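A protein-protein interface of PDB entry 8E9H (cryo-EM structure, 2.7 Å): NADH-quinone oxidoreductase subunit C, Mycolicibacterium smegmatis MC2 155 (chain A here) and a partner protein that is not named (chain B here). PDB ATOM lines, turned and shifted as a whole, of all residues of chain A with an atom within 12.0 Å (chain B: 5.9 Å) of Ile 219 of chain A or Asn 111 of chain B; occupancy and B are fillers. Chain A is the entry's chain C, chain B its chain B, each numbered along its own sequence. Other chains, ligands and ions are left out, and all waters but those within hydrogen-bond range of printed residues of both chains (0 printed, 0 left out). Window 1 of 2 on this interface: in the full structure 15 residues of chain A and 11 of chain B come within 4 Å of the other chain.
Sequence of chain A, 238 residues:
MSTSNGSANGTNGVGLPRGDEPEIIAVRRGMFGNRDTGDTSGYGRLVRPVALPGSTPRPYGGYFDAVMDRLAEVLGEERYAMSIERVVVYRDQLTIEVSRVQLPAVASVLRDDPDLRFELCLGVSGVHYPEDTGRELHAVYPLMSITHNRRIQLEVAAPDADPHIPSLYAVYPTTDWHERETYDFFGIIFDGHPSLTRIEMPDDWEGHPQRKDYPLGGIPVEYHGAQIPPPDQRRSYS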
ATOM      1  N   TRP A 205     -20.115 -30.974  19.318  1.00  0.00           N
ATOM      2  CA  TRP A 205     -20.337 -29.912  20.284  1.00  0.00           C
ATOM      3  C   TRP A 205     -19.670 -30.237  21.611  1.00  0.00           C
ATOM      4  O   TRP A 205     -19.551 -31.400  22.007  1.00  0.00           O
ATOM      5  CB  TRP A 205     -21.829 -29.693  20.503  1.00  0.00           C
ATOM      6  CG  TRP A 205     -22.148 -28.358  21.075  1.00  0.00           C
ATOM      7  CD1 TRP A 205     -22.401 -28.065  22.379  1.00  0.00           C
ATOM      8  CD2 TRP A 205     -22.246 -27.124  20.361  1.00  0.00           C
ATOM      9  NE1 TRP A 205     -22.653 -26.726  22.522  1.00  0.00           N
ATOM     10  CE2 TRP A 205     -22.563 -26.126  21.296  1.00  0.00           C
ATOM     11  CE3 TRP A 205     -22.096 -26.768  19.021  1.00  0.00           C
ATOM     12  CZ2 TRP A 205     -22.734 -24.797  20.935  1.00  0.00           C
ATOM     13  CZ3 TRP A 205     -22.267 -25.451  18.665  1.00  0.00           C
ATOM     14  CH2 TRP A 205     -22.582 -24.481  19.616  1.00  0.00           C
ATOM     15  N   PRO A 209     -25.802 -27.916  26.850  1.00  0.00           N
ATOM     16  CA  PRO A 209     -26.260 -26.525  26.986  1.00  0.00           C
ATOM     17  C   PRO A 209     -27.194 -26.251  28.151  1.00  0.00           C
ATOM     18  O   PRO A 209     -27.051 -25.210  28.801  1.00  0.00           O
ATOM     19  CB  PRO A 209     -26.951 -26.265  25.647  1.00  0.00           C
ATOM     20  CG  PRO A 209     -26.315 -27.189  24.705  1.00  0.00           C
ATOM     21  CD  PRO A 209     -25.985 -28.416  25.479  1.00  0.00           C
ATOM     22  N   TYR A 214     -23.597 -24.139  32.244  1.00  0.00           N
ATOM     23  CA  TYR A 214     -23.291 -23.821  30.856  1.00  0.00           C
ATOM     24  C   TYR A 214     -23.751 -22.404  30.541  1.00  0.00           C
ATOM     25  O   TYR A 214     -24.941 -22.103  30.700  1.00  0.00           O
ATOM     26  CB  TYR A 214     -23.977 -24.817  29.937  1.00  0.00           C
ATOM     27  CG  TYR A 214     -23.542 -24.735  28.497  1.00  0.00           C
ATOM     28  CD1 TYR A 214     -24.069 -23.779  27.647  1.00  0.00           C
ATOM     29  CD2 TYR A 214     -22.619 -25.626  27.982  1.00  0.00           C
ATOM     30  CE1 TYR A 214     -23.682 -23.708  26.332  1.00  0.00           C
ATOM     31  CE2 TYR A 214     -22.225 -25.562  26.668  1.00  0.00           C
ATOM     32  CZ  TYR A 214     -22.760 -24.601  25.848  1.00  0.00           C
ATOM     33  OH  TYR A 214     -22.369 -24.532  24.534  1.00  0.00           O
ATOM     34  N   PRO A 215     -22.873 -21.515  30.088  1.00  0.00           N
ATOM     35  CA  PRO A 215     -23.287 -20.129  29.858  1.00  0.00           C
ATOM     36  C   PRO A 215     -24.264 -20.013  28.700  1.00  0.00           C
ATOM     37  O   PRO A 215     -24.297 -20.837  27.785  1.00  0.00           O
ATOM     38  CB  PRO A 215     -21.970 -19.415  29.549  1.00  0.00           C
ATOM     39  CG  PRO A 215     -21.107 -20.469  28.986  1.00  0.00           C
ATOM     40  CD  PRO A 215     -21.468 -21.732  29.707  1.00  0.00           C
ATOM     41  N   LEU A 216     -25.071 -18.952  28.751  1.00  0.00           N
ATOM     42  CA  LEU A 216     -26.078 -18.742  27.720  1.00  0.00           C
ATOM     43  C   LEU A 216     -25.454 -18.612  26.340  1.00  0.00           C
ATOM     44  O   LEU A 216     -26.077 -18.988  25.342  1.00  0.00           O
ATOM     45  CB  LEU A 216     -26.899 -17.497  28.039  1.00  0.00           C
ATOM     46  CG  LEU A 216     -28.081 -17.229  27.111  1.00  0.00           C
ATOM     47  CD1 LEU A 216     -29.095 -18.347  27.198  1.00  0.00           C
ATOM     48  CD2 LEU A 216     -28.720 -15.904  27.451  1.00  0.00           C
ATOM     49  N   GLY A 217     -24.240 -18.077  26.256  1.00  0.00           N
ATOM     50  CA  GLY A 217     -23.556 -18.003  24.983  1.00  0.00           C
ATOM     51  C   GLY A 217     -24.073 -16.946  24.040  1.00  0.00           C
ATOM     52  O   GLY A 217     -23.882 -17.066  22.829  1.00  0.00           O
ATOM     53  N   GLY A 218     -24.724 -15.912  24.554  1.00  0.00           N
ATOM     54  CA  GLY A 218     -25.184 -14.829  23.717  1.00  0.00           C
ATOM     55  C   GLY A 218     -24.063 -13.870  23.373  1.00  0.00           C
ATOM     56  O   GLY A 218     -22.914 -14.018  23.788  1.00  0.00           O
ATOM     57  N   ILE A 219     -24.414 -12.862  22.588  1.00  0.00           N
ATOM     58  CA  ILE A 219     -23.486 -11.792  22.234  1.00  0.00           C
ATOM     59  C   ILE A 219     -24.142 -10.474  22.611  1.00  0.00           C
ATOM     60  O   ILE A 219     -25.377 -10.375  22.679  1.00  0.00           O
ATOM     61  CB  ILE A 219     -23.109 -11.826  20.736  1.00  0.00           C
ATOM     62  CG1 ILE A 219     -24.338 -11.575  19.863  1.00  0.00           C
ATOM     63  CG2 ILE A 219     -22.492 -13.152  20.384  1.00  0.00           C
ATOM     64  CD1 ILE A 219     -24.009 -11.374  18.411  1.00  0.00           C
ATOM     65  N   PRO A 220     -23.350  -9.437  22.867  1.00  0.00           N
ATOM     66  CA  PRO A 220     -23.942  -8.131  23.162  1.00  0.00           C
ATOM     67  C   PRO A 220     -24.786  -7.635  22.000  1.00  0.00           C
ATOM     68  O   PRO A 220     -24.432  -7.802  20.833  1.00  0.00           O
ATOM     69  CB  PRO A 220     -22.724  -7.234  23.397  1.00  0.00           C
ATOM     70  CG  PRO A 220     -21.625  -8.163  23.737  1.00  0.00           C
ATOM     71  CD  PRO A 220     -21.883  -9.400  22.951  1.00  0.00           C
ATOM     72  N   VAL A 221     -25.916  -7.017  22.332  1.00  0.00           N
ATOM     73  CA  VAL A 221     -26.774  -6.408  21.326  1.00  0.00           C
ATOM     74  C   VAL A 221     -26.228  -5.024  21.010  1.00  0.00           C
ATOM     75  O   VAL A 221     -26.044  -4.201  21.912  1.00  0.00           O
ATOM     76  CB  VAL A 221     -28.223  -6.335  21.816  1.00  0.00           C
ATOM     77  CG1 VAL A 221     -29.086  -5.638  20.793  1.00  0.00           C
ATOM     78  CG2 VAL A 221     -28.752  -7.722  22.100  1.00  0.00           C
ATOM     79  N   GLU A 222     -25.968  -4.766  19.734  1.00  0.00           N
ATOM     80  CA  GLU A 222     -25.313  -3.528  19.341  1.00  0.00           C
ATOM     81  C   GLU A 222     -26.298  -2.366  19.326  1.00  0.00           C
ATOM     82  O   GLU A 222     -27.491  -2.544  19.078  1.00  0.00           O
ATOM     83  CB  GLU A 222     -24.677  -3.685  17.963  1.00  0.00           C
ATOM     84  N   TYR A 223     -25.782  -1.167  19.581  1.00  0.00           N
ATOM     85  CA  TYR A 223     -26.551   0.062  19.530  1.00  0.00           C
ATOM     86  C   TYR A 223     -25.586   1.186  19.202  1.00  0.00           C
ATOM     87  O   TYR A 223     -24.390   1.098  19.487  1.00  0.00           O
ATOM     88  CB  TYR A 223     -27.245   0.364  20.859  1.00  0.00           C
ATOM     89  CG  TYR A 223     -28.382  -0.556  21.195  1.00  0.00           C
ATOM     90  CD1 TYR A 223     -29.637  -0.358  20.658  1.00  0.00           C
ATOM     91  CD2 TYR A 223     -28.201  -1.617  22.060  1.00  0.00           C
ATOM     92  CE1 TYR A 223     -30.676  -1.193  20.968  1.00  0.00           C
ATOM     93  CE2 TYR A 223     -29.234  -2.456  22.372  1.00  0.00           C
ATOM     94  CZ  TYR A 223     -30.470  -2.242  21.824  1.00  0.00           C
ATOM     95  OH  TYR A 223     -31.507  -3.086  22.137  1.00  0.00           O
ATOM     96  N   ALA A 226     -23.241   2.061  22.007  1.00  0.00           N
ATOM     97  CA  ALA A 226     -23.363   1.226  23.193  1.00  0.00           C
ATOM     98  C   ALA A 226     -23.676  -0.204  22.785  1.00  0.00           C
ATOM     99  O   ALA A 226     -23.833  -0.521  21.605  1.00  0.00           O
ATOM    100  CB  ALA A 226     -24.443   1.763  24.133  1.00  0.00           C
ATOM    101  N   GLN A 227     -23.754  -1.074  23.787  1.00  0.00           N
ATOM    102  CA  GLN A 227     -24.201  -2.438  23.567  1.00  0.00           C
ATOM    103  C   GLN A 227     -24.701  -3.016  24.880  1.00  0.00           C
ATOM    104  O   GLN A 227     -24.191  -2.693  25.954  1.00  0.00           O
ATOM    105  CB  GLN A 227     -23.091  -3.313  22.986  1.00  0.00           C
ATOM    106  CG  GLN A 227     -21.852  -3.399  23.839  1.00  0.00           C
ATOM    107  CD  GLN A 227     -20.726  -4.118  23.131  1.00  0.00           C
ATOM    108  OE1 GLN A 227     -20.741  -4.266  21.912  1.00  0.00           O
ATOM    109  NE2 GLN A 227     -19.742  -4.573  23.895  1.00  0.00           N
ATOM    110  N   ILE A 228     -25.706  -3.874  24.776  1.00  0.00           N
ATOM    111  CA  ILE A 228     -26.352  -4.488  25.931  1.00  0.00           C
ATOM    112  C   ILE A 228     -25.856  -5.925  26.040  1.00  0.00           C
ATOM    113  O   ILE A 228     -26.193  -6.744  25.177  1.00  0.00           O
ATOM    114  CB  ILE A 228     -27.881  -4.448  25.808  1.00  0.00           C
ATOM    115  CG1 ILE A 228     -28.360  -3.006  25.671  1.00  0.00           C
ATOM    116  CG2 ILE A 228     -28.523  -5.100  27.018  1.00  0.00           C
ATOM    117  CD1 ILE A 228     -29.847  -2.876  25.502  1.00  0.00           C
ATOM    118  N   PRO A 229     -25.095  -6.279  27.069  1.00  0.00           N
ATOM    119  CA  PRO A 229     -24.633  -7.657  27.199  1.00  0.00           C
ATOM    120  C   PRO A 229     -25.804  -8.621  27.244  1.00  0.00           C
ATOM    121  O   PRO A 229     -26.951  -8.206  27.457  1.00  0.00           O
ATOM    122  CB  PRO A 229     -23.870  -7.646  28.530  1.00  0.00           C
ATOM    123  CG  PRO A 229     -23.448  -6.248  28.695  1.00  0.00           C
ATOM    124  CD  PRO A 229     -24.566  -5.430  28.146  1.00  0.00           C
ATOM    125  N   PRO A 230     -25.559  -9.910  27.053  1.00  0.00           N
ATOM    126  CA  PRO A 230     -26.644 -10.885  27.114  1.00  0.00           C
ATOM    127  C   PRO A 230     -27.276 -10.894  28.492  1.00  0.00           C
ATOM    128  O   PRO A 230     -26.628 -10.531  29.483  1.00  0.00           O
ATOM    129  CB  PRO A 230     -25.941 -12.215  26.812  1.00  0.00           C
ATOM    130  CG  PRO A 230     -24.702 -11.840  26.107  1.00  0.00           C
ATOM    131  CD  PRO A 230     -24.279 -10.543  26.705  1.00  0.00           C
ATOM    132  N   PRO A 231     -28.539 -11.310  28.600  1.00  0.00           N
ATOM    133  CA  PRO A 231     -29.232 -11.227  29.891  1.00  0.00           C
ATOM    134  C   PRO A 231     -28.564 -12.014  31.000  1.00  0.00           C
ATOM    135  O   PRO A 231     -28.737 -11.658  32.172  1.00  0.00           O
ATOM    136  CB  PRO A 231     -30.618 -11.789  29.574  1.00  0.00           C
ATOM    137  CG  PRO A 231     -30.382 -12.706  28.434  1.00  0.00           C
ATOM    138  CD  PRO A 231     -29.341 -12.030  27.601  1.00  0.00           C
ATOM    139  N   ASP A 232     -27.818 -13.068  30.681  1.00  0.00           N
ATOM    140  CA  ASP A 232     -27.156 -13.854  31.713  1.00  0.00           C
ATOM    141  C   ASP A 232     -26.041 -13.085  32.401  1.00  0.00           C
ATOM    142  O   ASP A 232     -25.788 -13.316  33.587  1.00  0.00           O
ATOM    143  CB  ASP A 232     -26.590 -15.138  31.112  1.00  0.00           C
ATOM    144  CG  ASP A 232     -25.418 -14.879  30.200  1.00  0.00           C
ATOM    145  OD1 ASP A 232     -25.359 -13.778  29.621  1.00  0.00           O
ATOM    146  OD2 ASP A 232     -24.559 -15.772  30.057  1.00  0.00           O
ATOM    147  N   GLN A 233     -25.363 -12.190  31.685  1.00  0.00           N
ATOM    148  CA  GLN A 233     -24.312 -11.390  32.298  1.00  0.00           C
ATOM    149  C   GLN A 233     -24.878 -10.276  33.163  1.00  0.00           C
ATOM    150  O   GLN A 233     -24.268  -9.910  34.172  1.00  0.00           O
ATOM    151  CB  GLN A 233     -23.417 -10.788  31.221  1.00  0.00           C
ATOM    152  CG  GLN A 233     -22.772 -11.810  30.321  1.00  0.00           C
ATOM    153  CD  GLN A 233     -21.787 -11.183  29.367  1.00  0.00           C
ATOM    154  OE1 GLN A 233     -21.468 -10.002  29.479  1.00  0.00           O
ATOM    155  NE2 GLN A 233     -21.300 -11.970  28.419  1.00  0.00           N
ATOM    156  N   ARG A 234     -26.028  -9.731  32.791  1.00  0.00           N
ATOM    157  CA  ARG A 234     -26.577  -8.585  33.488  1.00  0.00           C
ATOM    158  C   ARG A 234     -27.248  -9.015  34.786  1.00  0.00           C
ATOM    159  O   ARG A 234     -27.373 -10.201  35.099  1.00  0.00           O
ATOM    160  CB  ARG A 234     -27.564  -7.846  32.591  1.00  0.00           C
ATOM    161  CG  ARG A 234     -26.977  -7.484  31.246  1.00  0.00           C
ATOM    162  CD  ARG A 234     -27.817  -6.466  30.519  1.00  0.00           C
ATOM    163  NE  ARG A 234     -29.235  -6.789  30.581  1.00  0.00           N
ATOM    164  CZ  ARG A 234     -29.877  -7.525  29.686  1.00  0.00           C
ATOM    165  NH1 ARG A 234     -29.251  -8.057  28.650  1.00  0.00           N
ATOM    166  NH2 ARG A 234     -31.180  -7.738  29.836  1.00  0.00           N
ATOM    167  N   SER B 106     -30.314 -10.885  12.716  1.00  0.00           N
ATOM    168  CA  SER B 106     -29.412 -10.646  13.834  1.00  0.00           C
ATOM    169  C   SER B 106     -29.524 -11.658  14.961  1.00  0.00           C
ATOM    170  O   SER B 106     -28.972 -11.404  16.033  1.00  0.00           O
ATOM    171  CB  SER B 106     -29.661  -9.244  14.397  1.00  0.00           C
ATOM    172  OG  SER B 106     -30.799  -9.242  15.236  1.00  0.00           O
ATOM    173  N   GLY B 107     -30.211 -12.778  14.777  1.00  0.00           N
ATOM    174  CA  GLY B 107     -30.484 -13.683  15.866  1.00  0.00           C
ATOM    175  C   GLY B 107     -31.719 -13.334  16.657  1.00  0.00           C
ATOM    176  O   GLY B 107     -32.202 -14.171  17.425  1.00  0.00           O
ATOM    177  N   GLY B 108     -32.248 -12.127  16.488  1.00  0.00           N
ATOM    178  CA  GLY B 108     -33.517 -11.785  17.093  1.00  0.00           C
ATOM    179  C   GLY B 108     -33.512 -11.987  18.590  1.00  0.00           C
ATOM    180  O   GLY B 108     -32.528 -11.710  19.283  1.00  0.00           O
ATOM    181  N   MET B 109     -34.635 -12.488  19.097  1.00  0.00           N
ATOM    182  CA  MET B 109     -34.802 -12.672  20.531  1.00  0.00           C
ATOM    183  C   MET B 109     -33.925 -13.788  21.073  1.00  0.00           C
ATOM    184  O   MET B 109     -33.718 -13.874  22.286  1.00  0.00           O
ATOM    185  CB  MET B 109     -36.267 -12.959  20.830  1.00  0.00           C
ATOM    186  CG  MET B 109     -36.593 -13.128  22.287  1.00  0.00           C
ATOM    187  SD  MET B 109     -38.347 -13.428  22.511  1.00  0.00           S
ATOM    188  CE  MET B 109     -38.467 -15.086  21.871  1.00  0.00           C
ATOM    189  N   PHE B 110     -33.402 -14.649  20.204  1.00  0.00           N
ATOM    190  CA  PHE B 110     -32.663 -15.828  20.643  1.00  0.00           C
ATOM    191  C   PHE B 110     -31.161 -15.553  20.634  1.00  0.00           C
ATOM    192  O   PHE B 110     -30.399 -16.052  19.809  1.00  0.00           O
ATOM    193  CB  PHE B 110     -33.029 -17.013  19.766  1.00  0.00           C
ATOM    194  CG  PHE B 110     -34.496 -17.257  19.698  1.00  0.00           C
ATOM    195  CD1 PHE B 110     -35.198 -17.610  20.827  1.00  0.00           C
ATOM    196  CD2 PHE B 110     -35.180 -17.119  18.510  1.00  0.00           C
ATOM    197  CE1 PHE B 110     -36.548 -17.818  20.774  1.00  0.00           C
ATOM    198  CE2 PHE B 110     -36.531 -17.334  18.454  1.00  0.00           C
ATOM    199  CZ  PHE B 110     -37.216 -17.686  19.587  1.00  0.00           C
ATOM    200  N   ASN B 111     -30.748 -14.724  21.588  1.00  0.00           N
ATOM    201  CA  ASN B 111     -29.343 -14.379  21.777  1.00  0.00           C
ATOM    202  C   ASN B 111     -28.703 -15.409  22.707  1.00  0.00           C
ATOM    203  O   ASN B 111     -28.523 -15.196  23.905  1.00  0.00           O
ATOM    204  CB  ASN B 111     -29.231 -12.968  22.330  1.00  0.00           C
ATOM    205  CG  ASN B 111     -27.814 -12.476  22.375  1.00  0.00           C
ATOM    206  OD1 ASN B 111     -26.893 -13.159  21.937  1.00  0.00           O
ATOM    207  ND2 ASN B 111     -27.627 -11.276  22.902  1.00  0.00           N
ATOM    208  N   ASN B 112     -28.359 -16.556  22.126  1.00  0.00           N
ATOM    209  CA  ASN B 112     -27.822 -17.659  22.906  1.00  0.00           C
ATOM    210  C   ASN B 112     -26.924 -18.519  22.029  1.00  0.00           C
ATOM    211  O   ASN B 112     -26.668 -18.209  20.865  1.00  0.00           O
ATOM    212  CB  ASN B 112     -28.946 -18.498  23.515  1.00  0.00           C
ATOM    213  CG  ASN B 112     -29.839 -19.115  22.470  1.00  0.00           C
ATOM    214  OD1 ASN B 112     -29.492 -19.169  21.296  1.00  0.00           O
ATOM    215  ND2 ASN B 112     -31.004 -19.577  22.891  1.00  0.00           N
ATOM    216  N   TYR B 113     -26.456 -19.621  22.614  1.00  0.00           N
ATOM    217  CA  TYR B 113     -25.489 -20.486  21.947  1.00  0.00           C
ATOM    218  C   TYR B 113     -26.033 -21.057  20.645  1.00  0.00           C
ATOM    219  O   TYR B 113     -25.316 -21.129  19.641  1.00  0.00           O
ATOM    220  CB  TYR B 113     -25.096 -21.628  22.884  1.00  0.00           C
ATOM    221  CG  TYR B 113     -26.258 -22.530  23.212  1.00  0.00           C
ATOM    222  CD1 TYR B 113     -27.190 -22.172  24.170  1.00  0.00           C
ATOM    223  CD2 TYR B 113     -26.442 -23.724  22.542  1.00  0.00           C
ATOM    224  CE1 TYR B 113     -28.259 -22.982  24.460  1.00  0.00           C
ATOM    225  CE2 TYR B 113     -27.509 -24.539  22.825  1.00  0.00           C
ATOM    226  CZ  TYR B 113     -28.417 -24.160  23.780  1.00  0.00           C
ATOM    227  OH  TYR B 113     -29.481 -24.976  24.068  1.00  0.00           O
ATOM    228  N   VAL B 115     -28.195 -20.283  18.291  1.00  0.00           N
ATOM    229  CA  VAL B 115     -28.522 -19.514  17.099  1.00  0.00           C
ATOM    230  C   VAL B 115     -27.273 -18.784  16.634  1.00  0.00           C
ATOM    231  O   VAL B 115     -26.409 -18.434  17.444  1.00  0.00           O
ATOM    232  CB  VAL B 115     -29.671 -18.524  17.362  1.00  0.00           C
ATOM    233  CG1 VAL B 115     -30.052 -17.807  16.088  1.00  0.00           C
ATOM    234  CG2 VAL B 115     -30.861 -19.250  17.933  1.00  0.00           C
ATOM    235  N   GLN B 117     -26.874 -15.825  15.392  1.00  0.00           N
ATOM    236  CA  GLN B 117     -26.827 -14.380  15.603  1.00  0.00           C
ATOM    237  C   GLN B 117     -26.645 -13.642  14.283  1.00  0.00           C
ATOM    238  O   GLN B 117     -25.746 -12.815  14.131  1.00  0.00           O
ATOM    239  CB  GLN B 117     -25.725 -13.997  16.591  1.00  0.00           C
ATOM    240  CG  GLN B 117     -25.868 -14.645  17.947  1.00  0.00           C
ATOM    241  CD  GLN B 117     -27.263 -14.504  18.504  1.00  0.00           C
ATOM    242  OE1 GLN B 117     -27.781 -13.397  18.627  1.00  0.00           O
ATOM    243  NE2 GLN B 117     -27.884 -15.626  18.830  1.00  0.00           N
ATOM    244  N   HIS B 121     -23.378 -13.950   9.257  1.00  0.00           N
ATOM    245  CA  HIS B 121     -22.208 -14.645   9.767  1.00  0.00           C
ATOM    246  C   HIS B 121     -21.724 -15.728   8.817  1.00  0.00           C
ATOM    247  O   HIS B 121     -20.569 -16.149   8.923  1.00  0.00           O
ATOM    248  CB  HIS B 121     -22.511 -15.260  11.131  1.00  0.00           C
ATOM    249  CG  HIS B 121     -22.390 -14.293  12.264  1.00  0.00           C
ATOM    250  ND1 HIS B 121     -22.905 -13.018  12.208  1.00  0.00           N
ATOM    251  CD2 HIS B 121     -21.800 -14.409  13.475  1.00  0.00           C
ATOM    252  CE1 HIS B 121     -22.646 -12.391  13.340  1.00  0.00           C
ATOM    253  NE2 HIS B 121     -21.976 -13.213  14.127  1.00  0.00           N
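Of chain B, only Asn 111 (2.4 Å) and Gln 117 (3.6 Å) come within 4 Å of Ile 219 of chain A. Of chain A, only Leu 216 (3.6 Å), Gly 218 (3.0 Å), Ile 219 (2.4 Å) and Val 221 (3.8 Å) come within 4 Å of Asn 111 of chain B. No residue of chain A comes within 4 Å of Gly 107 of chain B. No residue of chain A comes within 4 Å of Met 109 of chain B. No residue of chain A comes within 4 Å of Phe 110 of chain B. Asn 112 of chain B touches just these residues of chain A: Leu 216 (3.3 Å), Gly 217 (3.5 Å) and Gly 218 (3.9 Å). Printed residues of chain B within 4 Å of Gly 218 of chain A: Asn 111 and Asn 112. Printed residues of chain B within 4 Å of Gly 217 of chain A: Asn 112 (3.5 Å) and Tyr 113 (3.6 Å). Of the printed residues of chain B, Pro 209 of chain A touches Tyr 113. Of the printed residues of chain B, Leu 216 of chain A touches Asn 111 (3.6 Å), Asn 112 (3.3 Å) and Tyr 113 (2.8 Å). Of the printed residues of chain B, Val 221 of chain A touches Asn 111. The nearest residue of chain B that does not touch Ile 219 of chain A is His 121 of chain B (5.1 Å). The nearest printed residue of chain B that does not touch Leu 216 of chain A is Phe 110 of chain B (7.2 Å).
Among the printed residues, pairs that only touch across the chains: Pro 209 of chain A with Tyr 113 of chain B, Leu 216 of chain A with Asn 111 of chain B, Leu 216 of chain A with Asn 112 of chain B, Gly 217 of chain A with Asn 112 of chain B, Gly 217 of chain A with Tyr 113 of chain B, Gly 218 of chain A with Asn 111 of chain B, Gly 218 of chain A with Asn 112 of chain B, Ile 219 of chain A with Gln 117 of chain B and Val 221 of chain A with Asn 111 of chain B.
Of the 11 printed residues of chain B, 4 touch a printed residue of chain A. Printed residues of chain B that touch a printed residue of chain A: Asn 111, Asn 112, Tyr 113 and Gln 117. Hydrophobic or aromatic side chains of chain B that line the printed part of chain A: Tyr 113. Hydrophobic or aromatic side chains of chain A that line the printed part of chain B: Pro 209, Leu 216, Ile 219 and Val 221. Along chain A the printed residues that touch a printed residue of chain B span positions 209 to 221. Among the printed residues, no Asp or Glu carboxylate lies within 4 Å of a Lys or Arg side-chain nitrogen of the other chain.
The side-chain amide oxygen (OE1) of Gln 117 of chain B lies close to the backbone carbonyl oxygen (O) of Ser 106 of chain B (3.5 Å). The side-chain amide nitrogen (NE2) of Gln 117 of chain B is in hydrogen-bond range of the backbone carbonyl oxygen (O) of Phe 110 of chain B, at 2.7 Å. N of Val 115 of chain B lies within hydrogen-bond range of OD1 of Asn 112 of chain B (3.5 Å). The backbone NH (N) of Asn 112 of chain B sits close to the side-chain amide nitrogen (NE2) of Gln 117 of chain B (3.5 Å). N of Leu 216 of chain A is in hydrogen-bond range of OD2 of Asp 232 of chain A (3.5 Å). N of Val 221 of chain A is in hydrogen-bond range of O of Ile 228 of chain A (2.9 Å).
The side-chain amide nitrogen (ND2) of Asn 111 of chain B lies within hydrogen-bond range of the backbone carbonyl oxygen (O) of Ile 219 of chain A, 2.4 Å away. The backbone NH of Tyr 113 of chain B lies within hydrogen-bond range of the backbone carbonyl oxygen of Leu 216 of chain A, 2.8 Å away.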
